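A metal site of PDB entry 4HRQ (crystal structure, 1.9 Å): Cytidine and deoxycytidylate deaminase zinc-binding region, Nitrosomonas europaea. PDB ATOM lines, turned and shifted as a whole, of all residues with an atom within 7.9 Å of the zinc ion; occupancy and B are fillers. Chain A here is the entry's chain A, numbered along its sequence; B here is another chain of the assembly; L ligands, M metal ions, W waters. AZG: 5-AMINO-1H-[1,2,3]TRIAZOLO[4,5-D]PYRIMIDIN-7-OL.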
ATOM      1  N   PHE A  50     -29.709  20.068  -0.353  1.00  0.00           N
ATOM      2  CA  PHE A  50     -29.131  18.856   0.193  1.00  0.00           C
ATOM      3  C   PHE A  50     -30.129  18.081   1.038  1.00  0.00           C
ATOM      4  O   PHE A  50     -30.993  18.657   1.696  1.00  0.00           O
ATOM      5  CB  PHE A  50     -27.935  19.204   1.074  1.00  0.00           C
ATOM      6  CG  PHE A  50     -26.847  19.926   0.360  1.00  0.00           C
ATOM      7  CD1 PHE A  50     -25.857  19.231  -0.317  1.00  0.00           C
ATOM      8  CD2 PHE A  50     -26.798  21.313   0.388  1.00  0.00           C
ATOM      9  CE1 PHE A  50     -24.829  19.907  -0.957  1.00  0.00           C
ATOM     10  CE2 PHE A  50     -25.771  22.001  -0.243  1.00  0.00           C
ATOM     11  CZ  PHE A  50     -24.788  21.302  -0.915  1.00  0.00           C
ATOM     12  N   ASN A  68     -30.970  20.250   4.617  1.00  0.00           N
ATOM     13  CA  ASN A  68     -30.243  21.444   5.016  1.00  0.00           C
ATOM     14  C   ASN A  68     -31.244  22.478   5.486  1.00  0.00           C
ATOM     15  O   ASN A  68     -32.116  22.899   4.727  1.00  0.00           O
ATOM     16  CB  ASN A  68     -29.438  21.975   3.815  1.00  0.00           C
ATOM     17  CG  ASN A  68     -28.672  23.238   4.143  1.00  0.00           C
ATOM     18  OD1 ASN A  68     -27.482  23.342   3.859  1.00  0.00           O
ATOM     19  ND2 ASN A  68     -29.351  24.215   4.734  1.00  0.00           N
ATOM     20  N   SER A  76     -25.730  26.901  11.538  1.00  0.00           N
ATOM     21  CA  SER A  76     -24.756  26.461  10.539  1.00  0.00           C
ATOM     22  C   SER A  76     -24.447  24.967  10.616  1.00  0.00           C
ATOM     23  O   SER A  76     -23.953  24.386   9.648  1.00  0.00           O
ATOM     24  CB  SER A  76     -23.469  27.284  10.649  1.00  0.00           C
ATOM     25  OG  SER A  76     -22.894  27.176  11.928  1.00  0.00           O
ATOM     26  N   ALA A  77     -24.746  24.344  11.744  1.00  0.00           N
ATOM     27  CA  ALA A  77     -24.477  22.922  11.890  1.00  0.00           C
ATOM     28  C   ALA A  77     -25.618  22.051  11.345  1.00  0.00           C
ATOM     29  O   ALA A  77     -25.505  20.837  11.319  1.00  0.00           O
ATOM     30  CB  ALA A  77     -24.232  22.583  13.365  1.00  0.00           C
ATOM     31  N   ALA A  78     -26.706  22.682  10.899  1.00  0.00           N
ATOM     32  CA  ALA A  78     -27.867  21.947  10.398  1.00  0.00           C
ATOM     33  C   ALA A  78     -27.755  21.449   8.955  1.00  0.00           C
ATOM     34  O   ALA A  78     -28.580  21.800   8.100  1.00  0.00           O
ATOM     35  CB  ALA A  78     -29.131  22.795  10.564  1.00  0.00           C
ATOM     36  N   HIS A  79     -26.743  20.636   8.685  1.00  0.00           N
ATOM     37  CA  HIS A  79     -26.571  20.060   7.347  1.00  0.00           C
ATOM     38  C   HIS A  79     -27.443  18.812   7.271  1.00  0.00           C
ATOM     39  O   HIS A  79     -27.835  18.265   8.299  1.00  0.00           O
ATOM     40  CB  HIS A  79     -25.108  19.695   7.097  1.00  0.00           C
ATOM     41  CG  HIS A  79     -24.231  20.877   6.822  1.00  0.00           C
ATOM     42  ND1 HIS A  79     -22.994  20.758   6.206  1.00  0.00           N
ATOM     43  CD2 HIS A  79     -24.406  22.191   7.046  1.00  0.00           C
ATOM     44  CE1 HIS A  79     -22.457  21.954   6.059  1.00  0.00           C
ATOM     45  NE2 HIS A  79     -23.294  22.845   6.554  1.00  0.00           N
ATOM     46  N   ALA A  80     -27.768  18.377   6.058  1.00  0.00           N
ATOM     47  CA  ALA A  80     -28.594  17.189   5.830  1.00  0.00           C
ATOM     48  C   ALA A  80     -28.189  16.032   6.709  1.00  0.00           C
ATOM     49  O   ALA A  80     -28.986  15.477   7.468  1.00  0.00           O
ATOM     50  CB  ALA A  80     -28.499  16.749   4.380  1.00  0.00           C
ATOM     51  N   GLU A  81     -26.920  15.660   6.566  1.00  0.00           N
ATOM     52  CA  GLU A  81     -26.334  14.546   7.277  1.00  0.00           C
ATOM     53  C   GLU A  81     -26.503  14.635   8.786  1.00  0.00           C
ATOM     54  O   GLU A  81     -26.843  13.646   9.435  1.00  0.00           O
ATOM     55  CB  GLU A  81     -24.850  14.429   6.930  1.00  0.00           C
ATOM     56  CG  GLU A  81     -24.566  14.327   5.438  1.00  0.00           C
ATOM     57  CD  GLU A  81     -24.217  15.672   4.794  1.00  0.00           C
ATOM     58  OE1 GLU A  81     -25.000  16.627   4.905  1.00  0.00           O
ATOM     59  OE2 GLU A  81     -23.128  15.761   4.186  1.00  0.00           O
ATOM     60  N   ILE A  82     -26.275  15.815   9.339  1.00  0.00           N
ATOM     61  CA  ILE A  82     -26.393  16.013  10.783  1.00  0.00           C
ATOM     62  C   ILE A  82     -27.810  15.737  11.269  1.00  0.00           C
ATOM     63  O   ILE A  82     -28.010  15.023  12.247  1.00  0.00           O
ATOM     64  CB  ILE A  82     -25.993  17.465  11.196  1.00  0.00           C
ATOM     65  CG1 ILE A  82     -24.545  17.758  10.794  1.00  0.00           C
ATOM     66  CG2 ILE A  82     -26.146  17.638  12.709  1.00  0.00           C
ATOM     67  CD1 ILE A  82     -23.530  16.827  11.443  1.00  0.00           C
ATOM     68  N   THR A 109     -26.859  10.042   1.153  1.00  0.00           N
ATOM     69  CA  THR A 109     -26.768  11.487   1.044  1.00  0.00           C
ATOM     70  C   THR A 109     -26.703  11.979  -0.405  1.00  0.00           C
ATOM     71  O   THR A 109     -26.089  11.348  -1.270  1.00  0.00           O
ATOM     72  CB  THR A 109     -25.546  11.975   1.842  1.00  0.00           C
ATOM     73  OG1 THR A 109     -25.398  13.390   1.701  1.00  0.00           O
ATOM     74  CG2 THR A 109     -24.286  11.277   1.343  1.00  0.00           C
ATOM     75  N   ALA A 111     -25.074  14.338  -1.623  1.00  0.00           N
ATOM     76  CA  ALA A 111     -23.741  14.810  -2.004  1.00  0.00           C
ATOM     77  C   ALA A 111     -22.688  14.338  -1.001  1.00  0.00           C
ATOM     78  O   ALA A 111     -23.013  14.091   0.168  1.00  0.00           O
ATOM     79  CB  ALA A 111     -23.736  16.339  -2.071  1.00  0.00           C
ATOM     80  N   GLU A 112     -21.443  14.230  -1.451  1.00  0.00           N
ATOM     81  CA  GLU A 112     -20.364  13.798  -0.562  1.00  0.00           C
ATOM     82  C   GLU A 112     -20.289  14.778   0.609  1.00  0.00           C
ATOM     83  O   GLU A 112     -20.443  15.988   0.439  1.00  0.00           O
ATOM     84  CB  GLU A 112     -19.041  13.757  -1.331  1.00  0.00           C
ATOM     85  CG  GLU A 112     -19.053  12.709  -2.446  1.00  0.00           C
ATOM     86  CD  GLU A 112     -17.734  12.623  -3.212  1.00  0.00           C
ATOM     87  OE1 GLU A 112     -16.925  13.567  -3.108  1.00  0.00           O
ATOM     88  OE2 GLU A 112     -17.538  11.618  -3.926  1.00  0.00           O
ATOM     89  N   PRO A 113     -20.080  14.259   1.829  1.00  0.00           N
ATOM     90  CA  PRO A 113     -20.003  15.065   3.043  1.00  0.00           C
ATOM     91  C   PRO A 113     -18.896  16.103   3.173  1.00  0.00           C
ATOM     92  O   PRO A 113     -17.777  15.913   2.702  1.00  0.00           O
ATOM     93  CB  PRO A 113     -19.920  14.000   4.135  1.00  0.00           C
ATOM     94  CG  PRO A 113     -19.102  12.930   3.478  1.00  0.00           C
ATOM     95  CD  PRO A 113     -19.751  12.846   2.103  1.00  0.00           C
ATOM     96  N   CYS A 114     -19.220  17.222   3.817  1.00  0.00           N
ATOM     97  CA  CYS A 114     -18.254  18.276   4.057  1.00  0.00           C
ATOM     98  C   CYS A 114     -17.426  17.740   5.220  1.00  0.00           C
ATOM     99  O   CYS A 114     -17.767  16.704   5.791  1.00  0.00           O
ATOM    100  CB  CYS A 114     -18.943  19.583   4.476  1.00  0.00           C
ATOM    101  SG  CYS A 114     -19.574  19.601   6.181  1.00  0.00           S
ATOM    102  N   VAL A 115     -16.349  18.433   5.591  1.00  0.00           N
ATOM    103  CA  VAL A 115     -15.502  17.968   6.670  1.00  0.00           C
ATOM    104  C   VAL A 115     -16.274  17.775   7.985  1.00  0.00           C
ATOM    105  O   VAL A 115     -16.032  16.801   8.702  1.00  0.00           O
ATOM    106  CB  VAL A 115     -14.303  18.929   6.878  1.00  0.00           C
ATOM    107  CG1 VAL A 115     -14.800  20.331   7.190  1.00  0.00           C
ATOM    108  CG2 VAL A 115     -13.399  18.405   7.990  1.00  0.00           C
ATOM    109  N   MET A 116     -17.217  18.665   8.281  1.00  0.00           N
ATOM    110  CA  MET A 116     -17.999  18.541   9.503  1.00  0.00           C
ATOM    111  C   MET A 116     -18.778  17.218   9.527  1.00  0.00           C
ATOM    112  O   MET A 116     -18.655  16.430  10.470  1.00  0.00           O
ATOM    113  CB  MET A 116     -18.979  19.704   9.643  1.00  0.00           C
ATOM    114  CG  MET A 116     -19.942  19.562  10.821  1.00  0.00           C
ATOM    115  SD  MET A 116     -21.053  20.976  11.028  1.00  0.00           S
ATOM    116  CE  MET A 116     -22.191  20.736   9.657  1.00  0.00           C
ATOM    117  N   CYS A 117     -19.578  17.001   8.488  1.00  0.00           N
ATOM    118  CA  CYS A 117     -20.385  15.794   8.404  1.00  0.00           C
ATOM    119  C   CYS A 117     -19.547  14.534   8.289  1.00  0.00           C
ATOM    120  O   CYS A 117     -19.985  13.446   8.658  1.00  0.00           O
ATOM    121  CB  CYS A 117     -21.378  15.926   7.254  1.00  0.00           C
ATOM    122  SG  CYS A 117     -22.565  17.275   7.538  1.00  0.00           S
ATOM    123  N   PHE A 118     -18.338  14.692   7.764  1.00  0.00           N
ATOM    124  CA  PHE A 118     -17.391  13.590   7.612  1.00  0.00           C
ATOM    125  C   PHE A 118     -17.182  13.011   9.019  1.00  0.00           C
ATOM    126  O   PHE A 118     -17.309  11.807   9.243  1.00  0.00           O
ATOM    127  CB  PHE A 118     -16.079  14.144   7.026  1.00  0.00           C
ATOM    128  CG  PHE A 118     -14.911  13.207   7.136  1.00  0.00           C
ATOM    129  CD1 PHE A 118     -14.874  12.010   6.434  1.00  0.00           C
ATOM    130  CD2 PHE A 118     -13.811  13.541   7.930  1.00  0.00           C
ATOM    131  CE1 PHE A 118     -13.777  11.161   6.509  1.00  0.00           C
ATOM    132  CE2 PHE A 118     -12.713  12.703   8.014  1.00  0.00           C
ATOM    133  CZ  PHE A 118     -12.684  11.513   7.303  1.00  0.00           C
ATOM    134  N   ALA A 120     -19.091  13.559  11.652  1.00  0.00           N
ATOM    135  CA  ALA A 120     -20.383  13.132  12.196  1.00  0.00           C
ATOM    136  C   ALA A 120     -20.722  11.708  11.759  1.00  0.00           C
ATOM    137  O   ALA A 120     -21.298  10.935  12.523  1.00  0.00           O
ATOM    138  CB  ALA A 120     -21.481  14.088  11.739  1.00  0.00           C
ATOM    139  N   ASP A 144     -18.736  25.074  -0.343  1.00  0.00           N
ATOM    140  CA  ASP A 144     -17.476  24.580   0.200  1.00  0.00           C
ATOM    141  C   ASP A 144     -17.664  23.257   0.942  1.00  0.00           C
ATOM    142  O   ASP A 144     -18.624  23.089   1.691  1.00  0.00           O
ATOM    143  CB  ASP A 144     -16.931  25.624   1.184  1.00  0.00           C
ATOM    144  CG  ASP A 144     -15.418  25.613   1.274  1.00  0.00           C
ATOM    145  OD1 ASP A 144     -14.804  24.554   1.033  1.00  0.00           O
ATOM    146  OD2 ASP A 144     -14.846  26.667   1.602  1.00  0.00           O
ATOM    147  N   GLU A 145     -16.736  22.320   0.734  1.00  0.00           N
ATOM    148  CA  GLU A 145     -16.795  21.032   1.427  1.00  0.00           C
ATOM    149  C   GLU A 145     -15.872  21.113   2.635  1.00  0.00           C
ATOM    150  O   GLU A 145     -15.958  20.295   3.562  1.00  0.00           O
ATOM    151  CB  GLU A 145     -16.358  19.899   0.503  1.00  0.00           C
ATOM    152  CG  GLU A 145     -17.371  19.550  -0.592  1.00  0.00           C
ATOM    153  CD  GLU A 145     -18.540  18.717  -0.095  1.00  0.00           C
ATOM    154  OE1 GLU A 145     -19.116  19.044   0.967  1.00  0.00           O
ATOM    155  OE2 GLU A 145     -18.882  17.722  -0.767  1.00  0.00           O
ATOM    156  N   TRP B 123     -17.627  26.675   9.581  1.00  0.00           N
ATOM    157  CA  TRP B 123     -18.900  27.174   9.042  1.00  0.00           C
ATOM    158  C   TRP B 123     -19.662  28.105   9.981  1.00  0.00           C
ATOM    159  O   TRP B 123     -20.622  28.740   9.564  1.00  0.00           O
ATOM    160  CB  TRP B 123     -19.847  26.014   8.695  1.00  0.00           C
ATOM    161  CG  TRP B 123     -19.256  24.891   7.911  1.00  0.00           C
ATOM    162  CD1 TRP B 123     -19.431  23.556   8.147  1.00  0.00           C
ATOM    163  CD2 TRP B 123     -18.411  24.991   6.756  1.00  0.00           C
ATOM    164  NE1 TRP B 123     -18.751  22.819   7.209  1.00  0.00           N
ATOM    165  CE2 TRP B 123     -18.109  23.673   6.346  1.00  0.00           C
ATOM    166  CE3 TRP B 123     -17.869  26.069   6.032  1.00  0.00           C
ATOM    167  CZ2 TRP B 123     -17.293  23.399   5.245  1.00  0.00           C
ATOM    168  CZ3 TRP B 123     -17.062  25.792   4.935  1.00  0.00           C
ATOM    169  CH2 TRP B 123     -16.780  24.465   4.548  1.00  0.00           C
HETATM  170  C4  AZG L   1     -24.288  20.129   3.106  1.00  0.00           C
HETATM  171  N3  AZG L   1     -23.013  20.019   2.538  1.00  0.00           N
HETATM  172  C2  AZG L   1     -22.318  21.123   2.132  1.00  0.00           C
HETATM  173  N2  AZG L   1     -21.107  21.018   1.606  1.00  0.00           N
HETATM  174  N1  AZG L   1     -22.943  22.417   2.295  1.00  0.00           N
HETATM  175  C6  AZG L   1     -24.271  22.482   2.888  1.00  0.00           C
HETATM  176  O6  AZG L   1     -24.781  23.607   3.016  1.00  0.00           O
HETATM  177  C5  AZG L   1     -24.908  21.315   3.282  1.00  0.00           C
HETATM  178  N7  AZG L   1     -26.083  20.965   3.829  1.00  0.00           N
HETATM  179  N8  AZG L   1     -26.150  19.796   3.970  1.00  0.00           N
HETATM  180  N9  AZG L   1     -25.183  19.244   3.586  1.00  0.00           N
HETATM  181 ZN    ZN M   1     -21.851  18.919   6.013  1.00  0.00          ZN
HETATM  182  O   HOH W   1     -21.961  18.002   3.999  1.00  0.00           O
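The zinc ion is bound by a ring nitrogen (ND1) of His 79, water W1, the side-chain sulfur of Cys 117 and the side-chain sulfur of Cys 114.
The side-chain sulfur of Cys 114 lies close to the backbone NH of Met 116.
SG of Cys 114 lies close to NE1 of Trp 123 of chain B.
SG of Cys 117 sits close to OE1 of Glu 81 (3.6 Å).
N of Cys 114 lies close to OE1 of Glu 145, 3.4 Å away.
OE1 of Glu 145 is in hydrogen-bond range of N2 of the ligand.
N9 of the ligand lies close to OE1 of Glu 81, at 2.9 Å.
The backbone NH (N) of Ala 80 is in hydrogen-bond range of a nitrogen (N8) of the ligand.
The backbone carbonyl oxygen (O) of Asp 144 is in hydrogen-bond range of a nitrogen (N2) of the ligand, 3.2 Å away.
A nitrogen (N7) of the ligand sits at hydrogen-bond distance from the side-chain amide oxygen of Asn 68 (2.8 Å).
Water W1 lies within hydrogen-bond range of OE2 of Glu 81 (2.5 Å), N3 of the ligand (2.7 Å) and N of Cys 114 (2.9 Å).
Merely in contact with the zinc ion: Glu 81 (3.9 Å).
Four residues have an atom within 4 Å of the zinc ion: His 79, Glu 81, Cys 114 and Cys 117.
The nearest printed residue that does not touch the zinc ion is Met 116 (4.1 Å).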
